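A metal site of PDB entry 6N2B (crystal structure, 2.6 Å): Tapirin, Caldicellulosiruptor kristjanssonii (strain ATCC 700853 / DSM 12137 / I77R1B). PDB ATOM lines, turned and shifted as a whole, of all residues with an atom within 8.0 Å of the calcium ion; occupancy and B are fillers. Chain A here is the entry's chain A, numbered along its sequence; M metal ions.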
ATOM      1  N   PRO A 427      31.834 -35.296  20.329  1.00  0.00           N
ATOM      2  CA  PRO A 427      31.669 -34.967  18.905  1.00  0.00           C
ATOM      3  C   PRO A 427      31.727 -33.474  18.611  1.00  0.00           C
ATOM      4  O   PRO A 427      31.457 -32.627  19.459  1.00  0.00           O
ATOM      5  CB  PRO A 427      30.284 -35.524  18.584  1.00  0.00           C
ATOM      6  CG  PRO A 427      29.574 -35.548  19.903  1.00  0.00           C
ATOM      7  CD  PRO A 427      30.632 -35.933  20.894  1.00  0.00           C
ATOM      8  N   ALA A 428      32.063 -33.168  17.357  1.00  0.00           N
ATOM      9  CA  ALA A 428      32.031 -31.820  16.814  1.00  0.00           C
ATOM     10  C   ALA A 428      31.675 -31.916  15.340  1.00  0.00           C
ATOM     11  O   ALA A 428      32.129 -32.851  14.656  1.00  0.00           O
ATOM     12  CB  ALA A 428      33.376 -31.102  16.992  1.00  0.00           C
ATOM     13  N   ASP A 429      30.797 -30.985  14.851  1.00  0.00           N
ATOM     14  CA  ASP A 429      30.415 -30.792  13.451  1.00  0.00           C
ATOM     15  C   ASP A 429      30.966 -29.455  12.938  1.00  0.00           C
ATOM     16  O   ASP A 429      31.187 -28.544  13.729  1.00  0.00           O
ATOM     17  CB  ASP A 429      28.886 -30.840  13.199  1.00  0.00           C
ATOM     18  CG  ASP A 429      28.025 -30.487  14.455  1.00  0.00           C
ATOM     19  OD1 ASP A 429      27.761 -29.290  14.709  1.00  0.00           O
ATOM     20  OD2 ASP A 429      27.535 -31.423  15.137  1.00  0.00           O
ATOM     21  N   PRO A 430      31.219 -29.300  11.620  1.00  0.00           N
ATOM     22  CA  PRO A 430      31.626 -27.972  11.120  1.00  0.00           C
ATOM     23  C   PRO A 430      30.463 -27.013  10.969  1.00  0.00           C
ATOM     24  O   PRO A 430      30.717 -25.805  10.852  1.00  0.00           O
ATOM     25  CB  PRO A 430      32.262 -28.275   9.752  1.00  0.00           C
ATOM     26  CG  PRO A 430      32.439 -29.754   9.701  1.00  0.00           C
ATOM     27  CD  PRO A 430      31.356 -30.320  10.566  1.00  0.00           C
ATOM     28  N   VAL A 431      29.223 -27.502  10.979  1.00  0.00           N
ATOM     29  CA  VAL A 431      28.062 -26.614  11.104  1.00  0.00           C
ATOM     30  C   VAL A 431      28.153 -25.809  12.388  1.00  0.00           C
ATOM     31  O   VAL A 431      28.324 -26.372  13.481  1.00  0.00           O
ATOM     32  CB  VAL A 431      26.760 -27.432  11.069  1.00  0.00           C
ATOM     33  CG1 VAL A 431      25.578 -26.504  10.871  1.00  0.00           C
ATOM     34  CG2 VAL A 431      26.823 -28.481   9.972  1.00  0.00           C
ATOM     35  N   GLY A 432      27.989 -24.498  12.296  1.00  0.00           N
ATOM     36  CA  GLY A 432      28.061 -23.743  13.544  1.00  0.00           C
ATOM     37  C   GLY A 432      29.493 -23.632  14.055  1.00  0.00           C
ATOM     38  O   GLY A 432      30.455 -23.659  13.280  1.00  0.00           O
ATOM     39  N   ALA A 433      29.630 -23.502  15.369  1.00  0.00           N
ATOM     40  CA  ALA A 433      30.962 -23.423  15.972  1.00  0.00           C
ATOM     41  C   ALA A 433      31.750 -24.696  15.686  1.00  0.00           C
ATOM     42  O   ALA A 433      31.277 -25.801  15.978  1.00  0.00           O
ATOM     43  CB  ALA A 433      30.877 -23.178  17.473  1.00  0.00           C
ATOM     44  N   THR A 434      32.953 -24.542  15.120  1.00  0.00           N
ATOM     45  CA  THR A 434      33.685 -25.716  14.642  1.00  0.00           C
ATOM     46  C   THR A 434      34.305 -26.527  15.779  1.00  0.00           C
ATOM     47  O   THR A 434      34.733 -27.666  15.548  1.00  0.00           O
ATOM     48  CB  THR A 434      34.756 -25.306  13.601  1.00  0.00           C
ATOM     49  OG1 THR A 434      35.826 -24.594  14.223  1.00  0.00           O
ATOM     50  CG2 THR A 434      34.140 -24.409  12.519  1.00  0.00           C
ATOM     51  N   THR A 435      34.318 -25.988  16.995  1.00  0.00           N
ATOM     52  CA  THR A 435      34.743 -26.721  18.184  1.00  0.00           C
ATOM     53  C   THR A 435      33.633 -27.591  18.778  1.00  0.00           C
ATOM     54  O   THR A 435      33.931 -28.633  19.377  1.00  0.00           O
ATOM     55  CB  THR A 435      35.229 -25.743  19.249  1.00  0.00           C
ATOM     56  OG1 THR A 435      36.353 -25.014  18.734  1.00  0.00           O
ATOM     57  CG2 THR A 435      35.634 -26.474  20.536  1.00  0.00           C
ATOM     58  N   LEU A 436      32.378 -27.188  18.615  1.00  0.00           N
ATOM     59  CA  LEU A 436      31.252 -27.844  19.276  1.00  0.00           C
ATOM     60  C   LEU A 436      30.530 -28.820  18.359  1.00  0.00           C
ATOM     61  O   LEU A 436      30.596 -28.740  17.141  1.00  0.00           O
ATOM     62  CB  LEU A 436      30.233 -26.811  19.779  1.00  0.00           C
ATOM     63  CG  LEU A 436      30.698 -25.613  20.592  1.00  0.00           C
ATOM     64  CD1 LEU A 436      29.493 -24.718  20.926  1.00  0.00           C
ATOM     65  CD2 LEU A 436      31.405 -26.074  21.840  1.00  0.00           C
ATOM     66  N   GLY A 437      29.850 -29.770  18.988  1.00  0.00           N
ATOM     67  CA  GLY A 437      28.838 -30.541  18.304  1.00  0.00           C
ATOM     68  C   GLY A 437      27.539 -30.441  19.076  1.00  0.00           C
ATOM     69  O   GLY A 437      27.507 -30.052  20.233  1.00  0.00           O
ATOM     70  N   SER A 438      26.448 -30.794  18.407  1.00  0.00           N
ATOM     71  CA  SER A 438      25.180 -30.809  19.117  1.00  0.00           C
ATOM     72  C   SER A 438      24.220 -31.784  18.459  1.00  0.00           C
ATOM     73  O   SER A 438      24.376 -32.170  17.298  1.00  0.00           O
ATOM     74  CB  SER A 438      24.562 -29.405  19.191  1.00  0.00           C
ATOM     75  OG  SER A 438      24.395 -28.859  17.907  1.00  0.00           O
ATOM     76  N   VAL A 451      24.679 -29.573  23.806  1.00  0.00           N
ATOM     77  CA  VAL A 451      25.873 -29.044  23.164  1.00  0.00           C
ATOM     78  C   VAL A 451      27.092 -29.765  23.726  1.00  0.00           C
ATOM     79  O   VAL A 451      27.327 -29.768  24.934  1.00  0.00           O
ATOM     80  CB  VAL A 451      25.956 -27.517  23.347  1.00  0.00           C
ATOM     81  CG1 VAL A 451      27.280 -26.965  22.821  1.00  0.00           C
ATOM     82  CG2 VAL A 451      24.757 -26.864  22.629  1.00  0.00           C
ATOM     83  N   TYR A 452      27.867 -30.397  22.839  1.00  0.00           N
ATOM     84  CA  TYR A 452      29.082 -31.090  23.237  1.00  0.00           C
ATOM     85  C   TYR A 452      30.292 -30.220  22.917  1.00  0.00           C
ATOM     86  O   TYR A 452      30.416 -29.712  21.803  1.00  0.00           O
ATOM     87  CB  TYR A 452      29.211 -32.430  22.523  1.00  0.00           C
ATOM     88  CG  TYR A 452      28.091 -33.392  22.842  1.00  0.00           C
ATOM     89  CD1 TYR A 452      28.142 -34.192  23.977  1.00  0.00           C
ATOM     90  CD2 TYR A 452      26.972 -33.485  22.003  1.00  0.00           C
ATOM     91  CE1 TYR A 452      27.111 -35.085  24.254  1.00  0.00           C
ATOM     92  CE2 TYR A 452      25.937 -34.376  22.293  1.00  0.00           C
ATOM     93  CZ  TYR A 452      26.016 -35.173  23.414  1.00  0.00           C
ATOM     94  OH  TYR A 452      25.002 -36.047  23.717  1.00  0.00           O
ATOM     95  N   GLU A 461      30.734 -19.297  20.959  1.00  0.00           N
ATOM     96  CA  GLU A 461      30.513 -20.577  20.293  1.00  0.00           C
ATOM     97  C   GLU A 461      29.072 -21.054  20.422  1.00  0.00           C
ATOM     98  O   GLU A 461      28.495 -21.552  19.457  1.00  0.00           O
ATOM     99  CB  GLU A 461      31.468 -21.609  20.876  1.00  0.00           C
ATOM    100  CG  GLU A 461      32.896 -21.255  20.595  1.00  0.00           C
ATOM    101  CD  GLU A 461      33.834 -22.110  21.401  1.00  0.00           C
ATOM    102  OE1 GLU A 461      33.372 -22.664  22.433  1.00  0.00           O
ATOM    103  OE2 GLU A 461      35.016 -22.227  20.984  1.00  0.00           O
ATOM    104  N   THR A 464      26.739 -19.243  18.056  1.00  0.00           N
ATOM    105  CA  THR A 464      26.952 -19.790  16.720  1.00  0.00           C
ATOM    106  C   THR A 464      26.311 -21.162  16.577  1.00  0.00           C
ATOM    107  O   THR A 464      25.495 -21.387  15.677  1.00  0.00           O
ATOM    108  CB  THR A 464      28.457 -19.866  16.404  1.00  0.00           C
ATOM    109  OG1 THR A 464      29.028 -18.548  16.458  1.00  0.00           O
ATOM    110  CG2 THR A 464      28.685 -20.450  15.026  1.00  0.00           C
ATOM    111  N   GLU A 465      26.662 -22.099  17.464  1.00  0.00           N
ATOM    112  CA  GLU A 465      26.208 -23.481  17.308  1.00  0.00           C
ATOM    113  C   GLU A 465      24.689 -23.576  17.383  1.00  0.00           C
ATOM    114  O   GLU A 465      24.059 -24.209  16.518  1.00  0.00           O
ATOM    115  CB  GLU A 465      26.848 -24.375  18.367  1.00  0.00           C
ATOM    116  CG  GLU A 465      26.438 -25.825  18.244  1.00  0.00           C
ATOM    117  CD  GLU A 465      27.268 -26.553  17.217  1.00  0.00           C
ATOM    118  OE1 GLU A 465      28.236 -25.910  16.731  1.00  0.00           O
ATOM    119  OE2 GLU A 465      26.976 -27.728  16.888  1.00  0.00           O
ATOM    120  N   VAL A 466      24.074 -22.978  18.404  1.00  0.00           N
ATOM    121  CA  VAL A 466      22.632 -23.134  18.573  1.00  0.00           C
ATOM    122  C   VAL A 466      21.876 -22.598  17.351  1.00  0.00           C
ATOM    123  O   VAL A 466      21.007 -23.286  16.799  1.00  0.00           O
ATOM    124  CB  VAL A 466      22.165 -22.452  19.879  1.00  0.00           C
ATOM    125  CG1 VAL A 466      20.665 -22.298  19.907  1.00  0.00           C
ATOM    126  CG2 VAL A 466      22.619 -23.260  21.119  1.00  0.00           C
ATOM    127  N   SER A 468      22.820 -22.232  14.316  1.00  0.00           N
ATOM    128  CA  SER A 468      22.999 -23.028  13.113  1.00  0.00           C
ATOM    129  C   SER A 468      22.043 -24.218  13.093  1.00  0.00           C
ATOM    130  O   SER A 468      21.513 -24.570  12.030  1.00  0.00           O
ATOM    131  CB  SER A 468      24.443 -23.513  13.028  1.00  0.00           C
ATOM    132  OG  SER A 468      24.674 -24.486  14.039  1.00  0.00           O
ATOM    133  N   LYS A 469      21.806 -24.841  14.248  1.00  0.00           N
ATOM    134  CA  LYS A 469      20.983 -26.046  14.274  1.00  0.00           C
ATOM    135  C   LYS A 469      19.499 -25.712  14.286  1.00  0.00           C
ATOM    136  O   LYS A 469      18.696 -26.460  13.690  1.00  0.00           O
ATOM    137  CB  LYS A 469      21.318 -26.923  15.470  1.00  0.00           C
ATOM    138  CG  LYS A 469      22.777 -27.455  15.487  1.00  0.00           C
ATOM    139  CD  LYS A 469      23.087 -28.262  14.231  1.00  0.00           C
ATOM    140  CE  LYS A 469      24.345 -29.079  14.362  1.00  0.00           C
ATOM    141  NZ  LYS A 469      24.317 -30.147  15.406  1.00  0.00           N
HETATM  142 CA    CA M   1      29.347 -27.473  15.151  1.00  0.00          CA
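The calcium ion is bound by O of Val 431 (2.2 Å), OD1 of Asp 429 (2.5 Å), OE1 of Glu 465 (2.5 Å), O of Asp 429 (2.6 Å), O of Leu 436 (2.7 Å) and O of Ala 433 (2.7 Å). The calcium ion has six donor atoms within binding distance. Slightly farther from the calcium ion lies OE2 of Glu 465 (3.0 Å).
Gly 432 touches the calcium ion (C to CA, 3.997 Å). Within 4 Å of the calcium ion: Asp 429, Val 431, Gly 432, Ala 433, Leu 436 and Glu 465. The nearest printed residue that does not touch the calcium ion is Pro 430 (4.4 Å).
The side-chain carboxylate of Glu 465 is in hydrogen-bond range of the side-chain hydroxyl of Ser 438 (3.0 Å). The side-chain amino group of Lys 469 is in salt-bridge range of the side-chain carboxylate of Asp 429, at 3.5 Å. The backbone carbonyl oxygen (O) of Glu 465 is in hydrogen-bond range of the side-chain hydroxyl (OG) of Ser 468 (2.6 Å). OE2 of Glu 465 lies within salt-bridge range of NZ of Lys 469, 3.9 Å away.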
